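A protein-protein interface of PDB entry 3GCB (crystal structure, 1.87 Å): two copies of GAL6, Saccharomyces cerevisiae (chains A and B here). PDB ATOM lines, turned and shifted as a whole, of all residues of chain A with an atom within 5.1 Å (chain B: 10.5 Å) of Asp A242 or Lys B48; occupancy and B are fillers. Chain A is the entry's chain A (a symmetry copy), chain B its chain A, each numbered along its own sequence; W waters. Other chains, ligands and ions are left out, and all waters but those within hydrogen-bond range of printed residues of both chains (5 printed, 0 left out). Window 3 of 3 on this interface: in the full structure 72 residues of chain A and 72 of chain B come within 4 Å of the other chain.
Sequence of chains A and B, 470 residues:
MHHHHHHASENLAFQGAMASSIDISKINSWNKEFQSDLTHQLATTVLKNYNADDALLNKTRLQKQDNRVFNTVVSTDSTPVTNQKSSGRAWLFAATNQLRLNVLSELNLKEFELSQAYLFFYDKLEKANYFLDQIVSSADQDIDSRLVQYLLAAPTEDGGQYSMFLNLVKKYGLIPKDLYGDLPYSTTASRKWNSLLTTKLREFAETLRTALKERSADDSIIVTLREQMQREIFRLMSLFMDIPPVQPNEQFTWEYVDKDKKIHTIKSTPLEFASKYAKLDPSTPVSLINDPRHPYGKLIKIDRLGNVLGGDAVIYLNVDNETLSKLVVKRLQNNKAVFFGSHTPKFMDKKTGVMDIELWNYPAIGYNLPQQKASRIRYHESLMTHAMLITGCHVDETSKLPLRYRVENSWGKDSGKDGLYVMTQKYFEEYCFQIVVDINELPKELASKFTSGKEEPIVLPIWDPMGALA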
ATOM      1  N   PHE A 121      27.858 -30.756  -6.008  1.00  0.00           N
ATOM      2  CA  PHE A 121      27.618 -29.539  -6.795  1.00  0.00           C
ATOM      3  C   PHE A 121      27.467 -28.324  -5.894  1.00  0.00           C
ATOM      4  O   PHE A 121      28.151 -27.314  -6.067  1.00  0.00           O
ATOM      5  CB  PHE A 121      26.366 -29.696  -7.683  1.00  0.00           C
ATOM      6  CG  PHE A 121      26.081 -28.494  -8.558  1.00  0.00           C
ATOM      7  CD1 PHE A 121      25.282 -27.447  -8.089  1.00  0.00           C
ATOM      8  CD2 PHE A 121      26.628 -28.398  -9.834  1.00  0.00           C
ATOM      9  CE1 PHE A 121      25.038 -26.323  -8.883  1.00  0.00           C
ATOM     10  CE2 PHE A 121      26.396 -27.290 -10.632  1.00  0.00           C
ATOM     11  CZ  PHE A 121      25.595 -26.245 -10.156  1.00  0.00           C
ATOM     12  N   TYR A 180      20.073 -37.915 -10.091  1.00  0.00           N
ATOM     13  CA  TYR A 180      21.231 -37.065 -10.378  1.00  0.00           C
ATOM     14  C   TYR A 180      22.471 -37.853  -9.918  1.00  0.00           C
ATOM     15  O   TYR A 180      22.747 -37.955  -8.727  1.00  0.00           O
ATOM     16  CB  TYR A 180      21.026 -35.759  -9.576  1.00  0.00           C
ATOM     17  CG  TYR A 180      21.999 -34.637  -9.832  1.00  0.00           C
ATOM     18  CD1 TYR A 180      21.835 -33.776 -10.915  1.00  0.00           C
ATOM     19  CD2 TYR A 180      23.067 -34.424  -8.966  1.00  0.00           C
ATOM     20  CE1 TYR A 180      22.722 -32.723 -11.131  1.00  0.00           C
ATOM     21  CE2 TYR A 180      23.963 -33.376  -9.170  1.00  0.00           C
ATOM     22  CZ  TYR A 180      23.784 -32.532 -10.249  1.00  0.00           C
ATOM     23  OH  TYR A 180      24.684 -31.505 -10.424  1.00  0.00           O
ATOM     24  N   LEU A 183      27.200 -38.937 -13.690  1.00  0.00           N
ATOM     25  CA  LEU A 183      27.338 -38.916 -15.140  1.00  0.00           C
ATOM     26  C   LEU A 183      28.452 -37.983 -15.640  1.00  0.00           C
ATOM     27  O   LEU A 183      29.281 -38.392 -16.447  1.00  0.00           O
ATOM     28  CB  LEU A 183      26.005 -38.537 -15.821  1.00  0.00           C
ATOM     29  CG  LEU A 183      25.045 -39.704 -16.074  1.00  0.00           C
ATOM     30  CD1 LEU A 183      23.730 -39.232 -16.667  1.00  0.00           C
ATOM     31  CD2 LEU A 183      25.731 -40.688 -17.008  1.00  0.00           C
ATOM     32  N   PRO A 184      28.501 -36.726 -15.139  1.00  0.00           N
ATOM     33  CA  PRO A 184      29.547 -35.827 -15.630  1.00  0.00           C
ATOM     34  C   PRO A 184      30.960 -36.272 -15.351  1.00  0.00           C
ATOM     35  O   PRO A 184      31.279 -36.709 -14.249  1.00  0.00           O
ATOM     36  CB  PRO A 184      29.267 -34.522 -14.888  1.00  0.00           C
ATOM     37  CG  PRO A 184      27.793 -34.614 -14.523  1.00  0.00           C
ATOM     38  CD  PRO A 184      27.676 -36.053 -14.114  1.00  0.00           C
ATOM     39  N   TYR A 185      31.821 -35.987 -16.319  1.00  0.00           N
ATOM     40  CA  TYR A 185      33.241 -36.274 -16.227  1.00  0.00           C
ATOM     41  C   TYR A 185      33.845 -35.717 -14.925  1.00  0.00           C
ATOM     42  O   TYR A 185      34.621 -36.385 -14.250  1.00  0.00           O
ATOM     43  CB  TYR A 185      33.945 -35.610 -17.416  1.00  0.00           C
ATOM     44  CG  TYR A 185      35.450 -35.656 -17.332  1.00  0.00           C
ATOM     45  CD1 TYR A 185      36.154 -36.812 -17.701  1.00  0.00           C
ATOM     46  CD2 TYR A 185      36.171 -34.575 -16.826  1.00  0.00           C
ATOM     47  CE1 TYR A 185      37.539 -36.876 -17.559  1.00  0.00           C
ATOM     48  CE2 TYR A 185      37.542 -34.638 -16.675  1.00  0.00           C
ATOM     49  CZ  TYR A 185      38.220 -35.787 -17.044  1.00  0.00           C
ATOM     50  OH  TYR A 185      39.588 -35.834 -16.914  1.00  0.00           O
ATOM     51  N   SER A 238      28.125 -24.604 -13.985  1.00  0.00           N
ATOM     52  CA  SER A 238      27.094 -25.184 -14.858  1.00  0.00           C
ATOM     53  C   SER A 238      27.602 -25.755 -16.191  1.00  0.00           C
ATOM     54  O   SER A 238      26.854 -26.439 -16.895  1.00  0.00           O
ATOM     55  CB  SER A 238      25.933 -24.194 -15.077  1.00  0.00           C
ATOM     56  OG  SER A 238      26.248 -23.174 -16.016  1.00  0.00           O
ATOM     57  N   LEU A 239      28.846 -25.438 -16.552  1.00  0.00           N
ATOM     58  CA  LEU A 239      29.413 -25.964 -17.781  1.00  0.00           C
ATOM     59  C   LEU A 239      29.918 -27.376 -17.526  1.00  0.00           C
ATOM     60  O   LEU A 239      29.970 -28.198 -18.438  1.00  0.00           O
ATOM     61  CB  LEU A 239      30.587 -25.115 -18.267  1.00  0.00           C
ATOM     62  CG  LEU A 239      30.297 -23.703 -18.759  1.00  0.00           C
ATOM     63  CD1 LEU A 239      31.585 -23.078 -19.293  1.00  0.00           C
ATOM     64  CD2 LEU A 239      29.213 -23.756 -19.829  1.00  0.00           C
ATOM     65  N   PHE A 240      30.294 -27.651 -16.277  1.00  0.00           N
ATOM     66  CA  PHE A 240      30.850 -28.952 -15.929  1.00  0.00           C
ATOM     67  C   PHE A 240      29.894 -29.945 -15.263  1.00  0.00           C
ATOM     68  O   PHE A 240      30.144 -31.172 -15.270  1.00  0.00           O
ATOM     69  CB  PHE A 240      32.135 -28.749 -15.124  1.00  0.00           C
ATOM     70  CG  PHE A 240      33.199 -27.984 -15.877  1.00  0.00           C
ATOM     71  CD1 PHE A 240      33.128 -26.605 -15.997  1.00  0.00           C
ATOM     72  CD2 PHE A 240      34.227 -28.663 -16.526  1.00  0.00           C
ATOM     73  CE1 PHE A 240      34.045 -25.901 -16.751  1.00  0.00           C
ATOM     74  CE2 PHE A 240      35.162 -27.967 -17.289  1.00  0.00           C
ATOM     75  CZ  PHE A 240      35.072 -26.582 -17.406  1.00  0.00           C
ATOM     76  N   MET A 241      28.839 -29.417 -14.641  1.00  0.00           N
ATOM     77  CA  MET A 241      27.782 -30.232 -14.030  1.00  0.00           C
ATOM     78  C   MET A 241      26.494 -29.406 -14.179  1.00  0.00           C
ATOM     79  O   MET A 241      26.562 -28.191 -14.270  1.00  0.00           O
ATOM     80  CB  MET A 241      28.029 -30.481 -12.525  1.00  0.00           C
ATOM     81  CG  MET A 241      29.147 -31.460 -12.179  1.00  0.00           C
ATOM     82  SD  MET A 241      29.246 -31.756 -10.423  1.00  0.00           S
ATOM     83  CE  MET A 241      27.818 -32.750 -10.166  1.00  0.00           C
ATOM     84  N   ASP A 242      25.337 -30.058 -14.192  1.00  0.00           N
ATOM     85  CA  ASP A 242      24.075 -29.331 -14.277  1.00  0.00           C
ATOM     86  C   ASP A 242      23.617 -28.981 -12.864  1.00  0.00           C
ATOM     87  O   ASP A 242      23.912 -29.722 -11.914  1.00  0.00           O
ATOM     88  CB  ASP A 242      22.964 -30.223 -14.877  1.00  0.00           C
ATOM     89  CG  ASP A 242      23.271 -30.687 -16.277  1.00  0.00           C
ATOM     90  OD1 ASP A 242      23.796 -29.885 -17.070  1.00  0.00           O
ATOM     91  OD2 ASP A 242      22.954 -31.849 -16.593  1.00  0.00           O
ATOM     92  N   ILE A 243      22.845 -27.903 -12.712  1.00  0.00           N
ATOM     93  CA  ILE A 243      22.296 -27.584 -11.390  1.00  0.00           C
ATOM     94  C   ILE A 243      21.295 -28.732 -11.188  1.00  0.00           C
ATOM     95  O   ILE A 243      20.757 -29.254 -12.165  1.00  0.00           O
ATOM     96  CB  ILE A 243      21.560 -26.201 -11.395  1.00  0.00           C
ATOM     97  CG1 ILE A 243      21.189 -25.771  -9.951  1.00  0.00           C
ATOM     98  CG2 ILE A 243      20.346 -26.264 -12.309  1.00  0.00           C
ATOM     99  CD1 ILE A 243      20.735 -24.307  -9.808  1.00  0.00           C
ATOM    100  N   PRO A 244      21.149 -29.254  -9.950  1.00  0.00           N
ATOM    101  CA  PRO A 244      20.194 -30.347  -9.745  1.00  0.00           C
ATOM    102  C   PRO A 244      18.818 -30.012 -10.348  1.00  0.00           C
ATOM    103  O   PRO A 244      18.413 -28.850 -10.408  1.00  0.00           O
ATOM    104  CB  PRO A 244      20.189 -30.482  -8.222  1.00  0.00           C
ATOM    105  CG  PRO A 244      21.644 -30.276  -7.914  1.00  0.00           C
ATOM    106  CD  PRO A 244      21.979 -29.058  -8.748  1.00  0.00           C
ATOM    107  N   ILE B  27      20.422 -18.439  -8.491  1.00  0.00           N
ATOM    108  CA  ILE B  27      21.181 -19.354  -9.352  1.00  0.00           C
ATOM    109  C   ILE B  27      20.292 -20.096 -10.346  1.00  0.00           C
ATOM    110  O   ILE B  27      20.725 -20.390 -11.467  1.00  0.00           O
ATOM    111  CB  ILE B  27      22.093 -20.332  -8.553  1.00  0.00           C
ATOM    112  CG1 ILE B  27      21.260 -21.290  -7.683  1.00  0.00           C
ATOM    113  CG2 ILE B  27      23.130 -19.526  -7.748  1.00  0.00           C
ATOM    114  CD1 ILE B  27      22.077 -22.437  -7.030  1.00  0.00           C
ATOM    115  N   ASN B  28      19.039 -20.356  -9.976  1.00  0.00           N
ATOM    116  CA  ASN B  28      18.135 -21.031 -10.908  1.00  0.00           C
ATOM    117  C   ASN B  28      17.698 -20.074 -12.011  1.00  0.00           C
ATOM    118  O   ASN B  28      17.477 -20.490 -13.159  1.00  0.00           O
ATOM    119  CB  ASN B  28      16.947 -21.642 -10.185  1.00  0.00           C
ATOM    120  CG  ASN B  28      17.267 -23.007  -9.627  1.00  0.00           C
ATOM    121  OD1 ASN B  28      17.165 -24.028 -10.316  1.00  0.00           O
ATOM    122  ND2 ASN B  28      17.677 -23.035  -8.371  1.00  0.00           N
ATOM    123  N   ASN B  31      20.587 -19.852 -14.299  1.00  0.00           N
ATOM    124  CA  ASN B  31      20.627 -21.071 -15.101  1.00  0.00           C
ATOM    125  C   ASN B  31      19.698 -20.965 -16.337  1.00  0.00           C
ATOM    126  O   ASN B  31      20.062 -21.333 -17.465  1.00  0.00           O
ATOM    127  CB  ASN B  31      20.253 -22.276 -14.244  1.00  0.00           C
ATOM    128  CG  ASN B  31      20.518 -23.600 -14.952  1.00  0.00           C
ATOM    129  OD1 ASN B  31      21.647 -23.892 -15.334  1.00  0.00           O
ATOM    130  ND2 ASN B  31      19.472 -24.394 -15.141  1.00  0.00           N
ATOM    131  N   LYS B  32      18.493 -20.460 -16.106  1.00  0.00           N
ATOM    132  CA  LYS B  32      17.527 -20.294 -17.191  1.00  0.00           C
ATOM    133  C   LYS B  32      18.105 -19.377 -18.288  1.00  0.00           C
ATOM    134  O   LYS B  32      18.010 -19.678 -19.484  1.00  0.00           O
ATOM    135  CB  LYS B  32      16.236 -19.709 -16.621  1.00  0.00           C
ATOM    136  CG  LYS B  32      15.067 -19.819 -17.550  1.00  0.00           C
ATOM    137  CD  LYS B  32      13.819 -19.143 -16.956  1.00  0.00           C
ATOM    138  CE  LYS B  32      12.671 -19.157 -17.983  1.00  0.00           C
ATOM    139  NZ  LYS B  32      11.734 -18.000 -17.810  1.00  0.00           N
ATOM    140  N   PHE B  34      21.363 -18.698 -18.912  1.00  0.00           N
ATOM    141  CA  PHE B  34      22.495 -19.351 -19.566  1.00  0.00           C
ATOM    142  C   PHE B  34      22.033 -20.403 -20.557  1.00  0.00           C
ATOM    143  O   PHE B  34      22.560 -20.480 -21.668  1.00  0.00           O
ATOM    144  CB  PHE B  34      23.444 -19.954 -18.532  1.00  0.00           C
ATOM    145  CG  PHE B  34      24.160 -18.917 -17.687  1.00  0.00           C
ATOM    146  CD1 PHE B  34      24.522 -17.691 -18.230  1.00  0.00           C
ATOM    147  CD2 PHE B  34      24.443 -19.158 -16.349  1.00  0.00           C
ATOM    148  CE1 PHE B  34      25.144 -16.728 -17.453  1.00  0.00           C
ATOM    149  CE2 PHE B  34      25.058 -18.199 -15.582  1.00  0.00           C
ATOM    150  CZ  PHE B  34      25.408 -16.984 -16.131  1.00  0.00           C
ATOM    151  N   GLN B  35      21.009 -21.165 -20.190  1.00  0.00           N
ATOM    152  CA  GLN B  35      20.492 -22.194 -21.087  1.00  0.00           C
ATOM    153  C   GLN B  35      19.848 -21.634 -22.372  1.00  0.00           C
ATOM    154  O   GLN B  35      19.691 -22.357 -23.354  1.00  0.00           O
ATOM    155  CB  GLN B  35      19.532 -23.133 -20.346  1.00  0.00           C
ATOM    156  CG  GLN B  35      20.188 -24.005 -19.279  1.00  0.00           C
ATOM    157  CD  GLN B  35      21.273 -24.946 -19.834  1.00  0.00           C
ATOM    158  OE1 GLN B  35      21.193 -25.426 -20.975  1.00  0.00           O
ATOM    159  NE2 GLN B  35      22.284 -25.230 -19.007  1.00  0.00           N
ATOM    160  N   THR B  39      25.759 -21.194 -27.236  1.00  0.00           N
ATOM    161  CA  THR B  39      27.161 -21.546 -26.986  1.00  0.00           C
ATOM    162  C   THR B  39      27.241 -22.269 -25.646  1.00  0.00           C
ATOM    163  O   THR B  39      27.964 -23.251 -25.513  1.00  0.00           O
ATOM    164  CB  THR B  39      28.091 -20.325 -27.005  1.00  0.00           C
ATOM    165  OG1 THR B  39      27.780 -19.533 -28.169  1.00  0.00           O
ATOM    166  CG2 THR B  39      29.573 -20.776 -27.070  1.00  0.00           C
ATOM    167  N   HIS B  40      26.464 -21.793 -24.671  1.00  0.00           N
ATOM    168  CA  HIS B  40      26.401 -22.404 -23.348  1.00  0.00           C
ATOM    169  C   HIS B  40      25.811 -23.823 -23.437  1.00  0.00           C
ATOM    170  O   HIS B  40      26.305 -24.761 -22.810  1.00  0.00           O
ATOM    171  CB  HIS B  40      25.524 -21.564 -22.432  1.00  0.00           C
ATOM    172  CG  HIS B  40      25.628 -21.953 -20.996  1.00  0.00           C
ATOM    173  ND1 HIS B  40      26.601 -21.446 -20.166  1.00  0.00           N
ATOM    174  CD2 HIS B  40      24.901 -22.821 -20.249  1.00  0.00           C
ATOM    175  CE1 HIS B  40      26.479 -21.987 -18.968  1.00  0.00           C
ATOM    176  NE2 HIS B  40      25.459 -22.822 -18.993  1.00  0.00           N
ATOM    177  N   GLN B  41      24.711 -23.953 -24.168  1.00  0.00           N
ATOM    178  CA  GLN B  41      24.095 -25.260 -24.354  1.00  0.00           C
ATOM    179  C   GLN B  41      25.095 -26.257 -24.940  1.00  0.00           C
ATOM    180  O   GLN B  41      25.174 -27.400 -24.499  1.00  0.00           O
ATOM    181  CB  GLN B  41      22.906 -25.128 -25.290  1.00  0.00           C
ATOM    182  CG  GLN B  41      21.761 -24.313 -24.715  1.00  0.00           C
ATOM    183  CD  GLN B  41      20.631 -24.201 -25.715  1.00  0.00           C
ATOM    184  OE1 GLN B  41      20.298 -25.178 -26.388  1.00  0.00           O
ATOM    185  NE2 GLN B  41      20.055 -23.013 -25.843  1.00  0.00           N
ATOM    186  N   LEU B  42      25.870 -25.822 -25.931  1.00  0.00           N
ATOM    187  CA  LEU B  42      26.867 -26.695 -26.548  1.00  0.00           C
ATOM    188  C   LEU B  42      28.003 -26.983 -25.569  1.00  0.00           C
ATOM    189  O   LEU B  42      28.431 -28.128 -25.432  1.00  0.00           O
ATOM    190  CB  LEU B  42      27.438 -26.046 -27.801  1.00  0.00           C
ATOM    191  CG  LEU B  42      28.554 -26.850 -28.477  1.00  0.00           C
ATOM    192  CD1 LEU B  42      28.035 -28.241 -28.869  1.00  0.00           C
ATOM    193  CD2 LEU B  42      29.097 -26.091 -29.699  1.00  0.00           C
ATOM    194  N   ALA B  43      28.478 -25.958 -24.874  1.00  0.00           N
ATOM    195  CA  ALA B  43      29.576 -26.117 -23.940  1.00  0.00           C
ATOM    196  C   ALA B  43      29.288 -27.089 -22.803  1.00  0.00           C
ATOM    197  O   ALA B  43      30.106 -27.952 -22.494  1.00  0.00           O
ATOM    198  CB  ALA B  43      30.009 -24.745 -23.393  1.00  0.00           C
ATOM    199  N   THR B  44      28.135 -26.953 -22.160  1.00  0.00           N
ATOM    200  CA  THR B  44      27.810 -27.842 -21.049  1.00  0.00           C
ATOM    201  C   THR B  44      27.621 -29.287 -21.524  1.00  0.00           C
ATOM    202  O   THR B  44      27.943 -30.224 -20.804  1.00  0.00           O
ATOM    203  CB  THR B  44      26.601 -27.319 -20.209  1.00  0.00           C
ATOM    204  OG1 THR B  44      26.446 -28.151 -19.054  1.00  0.00           O
ATOM    205  CG2 THR B  44      25.304 -27.279 -21.008  1.00  0.00           C
ATOM    206  N   THR B  45      27.132 -29.466 -22.750  1.00  0.00           N
ATOM    207  CA  THR B  45      26.958 -30.814 -23.270  1.00  0.00           C
ATOM    208  C   THR B  45      28.330 -31.469 -23.419  1.00  0.00           C
ATOM    209  O   THR B  45      28.552 -32.569 -22.902  1.00  0.00           O
ATOM    210  CB  THR B  45      26.212 -30.809 -24.623  1.00  0.00           C
ATOM    211  OG1 THR B  45      24.878 -30.335 -24.416  1.00  0.00           O
ATOM    212  CG2 THR B  45      26.131 -32.220 -25.222  1.00  0.00           C
ATOM    213  N   VAL B  46      29.258 -30.751 -24.047  1.00  0.00           N
ATOM    214  CA  VAL B  46      30.607 -31.250 -24.299  1.00  0.00           C
ATOM    215  C   VAL B  46      31.457 -31.409 -23.032  1.00  0.00           C
ATOM    216  O   VAL B  46      32.087 -32.455 -22.819  1.00  0.00           O
ATOM    217  CB  VAL B  46      31.342 -30.358 -25.330  1.00  0.00           C
ATOM    218  CG1 VAL B  46      32.772 -30.832 -25.534  1.00  0.00           C
ATOM    219  CG2 VAL B  46      30.606 -30.398 -26.658  1.00  0.00           C
ATOM    220  N   LEU B  47      31.425 -30.401 -22.171  1.00  0.00           N
ATOM    221  CA  LEU B  47      32.215 -30.416 -20.941  1.00  0.00           C
ATOM    222  C   LEU B  47      31.775 -31.393 -19.840  1.00  0.00           C
ATOM    223  O   LEU B  47      32.512 -31.595 -18.884  1.00  0.00           O
ATOM    224  CB  LEU B  47      32.426 -28.990 -20.430  1.00  0.00           C
ATOM    225  CG  LEU B  47      33.246 -28.117 -21.412  1.00  0.00           C
ATOM    226  CD1 LEU B  47      33.264 -26.669 -20.946  1.00  0.00           C
ATOM    227  CD2 LEU B  47      34.674 -28.646 -21.555  1.00  0.00           C
ATOM    228  N   LYS B  48      30.594 -32.002 -19.983  1.00  0.00           N
ATOM    229  CA  LYS B  48      30.148 -33.027 -19.037  1.00  0.00           C
ATOM    230  C   LYS B  48      30.663 -34.378 -19.574  1.00  0.00           C
ATOM    231  O   LYS B  48      30.674 -35.379 -18.866  1.00  0.00           O
ATOM    232  CB  LYS B  48      28.612 -33.098 -18.934  1.00  0.00           C
ATOM    233  CG  LYS B  48      27.973 -31.995 -18.058  1.00  0.00           C
ATOM    234  CD  LYS B  48      26.504 -32.302 -17.757  1.00  0.00           C
ATOM    235  CE  LYS B  48      25.594 -32.191 -18.982  1.00  0.00           C
ATOM    236  NZ  LYS B  48      25.264 -30.774 -19.302  1.00  0.00           N
ATOM    237  N   ASN B  49      31.113 -34.391 -20.820  1.00  0.00           N
ATOM    238  CA  ASN B  49      31.601 -35.613 -21.459  1.00  0.00           C
ATOM    239  C   ASN B  49      33.118 -35.785 -21.458  1.00  0.00           C
ATOM    240  O   ASN B  49      33.624 -36.902 -21.314  1.00  0.00           O
ATOM    241  CB  ASN B  49      31.116 -35.678 -22.924  1.00  0.00           C
ATOM    242  CG  ASN B  49      29.609 -35.842 -23.043  1.00  0.00           C
ATOM    243  OD1 ASN B  49      28.957 -36.294 -22.126  1.00  0.00           O
ATOM    244  ND2 ASN B  49      29.059 -35.452 -24.177  1.00  0.00           N
ATOM    245  N   TYR B  50      33.866 -34.709 -21.641  1.00  0.00           N
ATOM    246  CA  TYR B  50      35.324 -34.828 -21.706  1.00  0.00           C
ATOM    247  C   TYR B  50      36.054 -33.819 -20.876  1.00  0.00           C
ATOM    248  O   TYR B  50      35.532 -32.756 -20.606  1.00  0.00           O
ATOM    249  CB  TYR B  50      35.823 -34.634 -23.150  1.00  0.00           C
ATOM    250  CG  TYR B  50      35.388 -35.721 -24.090  1.00  0.00           C
ATOM    251  CD1 TYR B  50      36.051 -36.945 -24.103  1.00  0.00           C
ATOM    252  CD2 TYR B  50      34.285 -35.548 -24.943  1.00  0.00           C
ATOM    253  CE1 TYR B  50      35.637 -37.972 -24.935  1.00  0.00           C
ATOM    254  CE2 TYR B  50      33.859 -36.569 -25.781  1.00  0.00           C
ATOM    255  CZ  TYR B  50      34.540 -37.787 -25.780  1.00  0.00           C
ATOM    256  OH  TYR B  50      34.171 -38.820 -26.622  1.00  0.00           O
ATOM    257  N   ASN B  51      37.297 -34.144 -20.542  1.00  0.00           N
ATOM    258  CA  ASN B  51      38.179 -33.241 -19.820  1.00  0.00           C
ATOM    259  C   ASN B  51      38.247 -31.965 -20.678  1.00  0.00           C
ATOM    260  O   ASN B  51      38.345 -32.045 -21.900  1.00  0.00           O
ATOM    261  CB  ASN B  51      39.566 -33.889 -19.702  1.00  0.00           C
ATOM    262  CG  ASN B  51      40.561 -33.020 -18.959  1.00  0.00           C
ATOM    263  OD1 ASN B  51      40.890 -33.276 -17.798  1.00  0.00           O
ATOM    264  ND2 ASN B  51      41.070 -32.011 -19.631  1.00  0.00           N
ATOM    265  N   ALA B  52      38.211 -30.796 -20.037  1.00  0.00           N
ATOM    266  CA  ALA B  52      38.234 -29.528 -20.765  1.00  0.00           C
ATOM    267  C   ALA B  52      39.394 -29.392 -21.725  1.00  0.00           C
ATOM    268  O   ALA B  52      39.217 -28.894 -22.822  1.00  0.00           O
ATOM    269  CB  ALA B  52      38.196 -28.321 -19.798  1.00  0.00           C
ATOM    270  N   ASP B  53      40.586 -29.828 -21.325  1.00  0.00           N
ATOM    271  CA  ASP B  53      41.739 -29.725 -22.213  1.00  0.00           C
ATOM    272  C   ASP B  53      41.608 -30.608 -23.444  1.00  0.00           C
ATOM    273  O   ASP B  53      42.054 -30.235 -24.524  1.00  0.00           O
ATOM    274  CB  ASP B  53      43.043 -30.030 -21.477  1.00  0.00           C
ATOM    275  CG  ASP B  53      43.474 -28.896 -20.557  1.00  0.00           C
ATOM    276  OD1 ASP B  53      43.211 -27.703 -20.844  1.00  0.00           O
ATOM    277  OD2 ASP B  53      44.086 -29.210 -19.538  1.00  0.00           O
ATOM    278  N   ALA B  55      38.675 -31.617 -24.716  1.00  0.00           N
ATOM    279  CA  ALA B  55      37.579 -31.042 -25.468  1.00  0.00           C
ATOM    280  C   ALA B  55      37.989 -29.797 -26.236  1.00  0.00           C
ATOM    281  O   ALA B  55      37.643 -29.638 -27.421  1.00  0.00           O
ATOM    282  CB  ALA B  55      36.411 -30.696 -24.506  1.00  0.00           C
ATOM    283  N   LEU B  56      38.756 -28.936 -25.573  1.00  0.00           N
ATOM    284  CA  LEU B  56      39.125 -27.652 -26.160  1.00  0.00           C
ATOM    285  C   LEU B  56      40.417 -27.512 -26.934  1.00  0.00           C
ATOM    286  O   LEU B  56      40.684 -26.430 -27.467  1.00  0.00           O
ATOM    287  CB  LEU B  56      38.999 -26.547 -25.105  1.00  0.00           C
ATOM    288  CG  LEU B  56      37.618 -26.456 -24.436  1.00  0.00           C
ATOM    289  CD1 LEU B  56      37.641 -25.438 -23.301  1.00  0.00           C
ATOM    290  CD2 LEU B  56      36.538 -26.077 -25.479  1.00  0.00           C
ATOM    291  N   ILE B 365      34.469 -20.679 -24.723  1.00  0.00           N
ATOM    292  CA  ILE B 365      33.505 -20.934 -23.646  1.00  0.00           C
ATOM    293  C   ILE B 365      33.463 -19.720 -22.722  1.00  0.00           C
ATOM    294  O   ILE B 365      32.960 -19.790 -21.609  1.00  0.00           O
ATOM    295  CB  ILE B 365      33.793 -22.229 -22.836  1.00  0.00           C
ATOM    296  CG1 ILE B 365      35.128 -22.136 -22.094  1.00  0.00           C
ATOM    297  CG2 ILE B 365      33.784 -23.468 -23.783  1.00  0.00           C
ATOM    298  CD1 ILE B 365      35.242 -23.137 -20.979  1.00  0.00           C
HETATM  299  O   HOH W   1      22.555 -26.487 -15.160  1.00  0.00           O
HETATM  300  O   HOH W   2      16.923 -26.713  -9.658  1.00  0.00           O
HETATM  301  O   HOH W   3      23.575 -23.696 -17.426  1.00  0.00           O
HETATM  302  O   HOH W   4      32.309 -32.382 -16.160  1.00  0.00           O
HETATM  303  O   HOH W   5      24.278 -27.025 -17.107  1.00  0.00           O
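The side-chain hydroxyl (OG) of Ser A238 sits at hydrogen-bond distance from a ring nitrogen (NE2) of His B40.
The side-chain hydroxyl of Thr B44 is in hydrogen-bond range of the backbone carbonyl oxygen of Ser A238 (2.8 Å).
The backbone NH (N) of Tyr A185 sits at hydrogen-bond distance from the backbone carbonyl oxygen (O) of Lys B48 (2.9 Å).
NZ of Lys B48 is in salt-bridge range of OD1 of Asp A242 (2.8 Å).
The side-chain amide oxygen of Asn B51 is in hydrogen-bond range of the side-chain hydroxyl of Tyr A185.
N of Asp B53 lies close to ND2 of Asn B51.
The backbone carbonyl oxygen (O) of Asp A242 sits at hydrogen-bond distance from the side-chain hydroxyl (OH) of Tyr A180 (2.4 Å).
No position is printed for both chains.
Of the 17 pairs that touch across the chains among the printed residues, none has its exchanged pair printed and touching as well.
Printed residues of chain A that touch a printed residue of chain B: Pro A184, Tyr A185, Ser A238, Leu A239, Phe A240, Asp A242 and Ile A243.
Hydrophobic or aromatic side chains of chain A that line the printed part of chain B: Tyr A185, Leu A239, Phe A240 and Ile A243.
Among the printed residues, 17 pairs touch across the chains.
Among the printed residues, Asp or Glu carboxylates within 4 Å of a Lys or Arg side-chain nitrogen of the other chain: Asp A242 with Lys B48.
Water W4 bridges O of Phe A240 (2.6 Å) and O of Leu B47 (2.8 Å).
Water W2 bridges O of Pro A244 and OD1 of Asn B28.
Water W1 lies within hydrogen-bond range of the side-chain amide oxygen of Asn B31 (2.8 Å) and the backbone NH of Ile A243 (2.8 Å).
Among the printed residues, merely in contact across the chains: Pro A184 with Lys B48 (3.5 Å), Leu A239 with His B40 (3.4 Å), Leu A239 with Ala B43 (3.8 Å), Leu A239 with Thr B44 (3.4 Å), Leu A239 with Leu B47 (3.3 Å), Phe A240 with Leu B47 (3.98 Å), Phe A240 with Lys B48 (3.6 Å), Phe A240 with Ala B52 (3.95 Å), Asp A242 with Thr B44 (3.7 Å), Ile A243 with Ile B27 (3.6 Å), Ile A243 with Asn B28 (3.6 Å) and Ile A243 with Asn B31 (3.5 Å).
Asp A242 touches just these residues of chain B: Thr B44 and Lys B48.
Of chain B, only Lys B48 (3.5 Å) comes within 4 Å of Pro A184.
Ile A243 touches just these residues of chain B: Ile B27 (3.6 Å), Asn B28 (3.6 Å) and Asn B31 (3.5 Å).
No residue of chain B comes within 4 Å of Pro A244.
Of the printed residues of chain B, Tyr A185 touches Lys B48 (2.9 Å) and Asn B51 (3.0 Å).
Of the printed residues of chain A, Ile B27 touches Ile A243 (3.6 Å).
Of the printed residues of chain B, Phe A240 touches Leu B47, Lys B48 and Ala B52.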
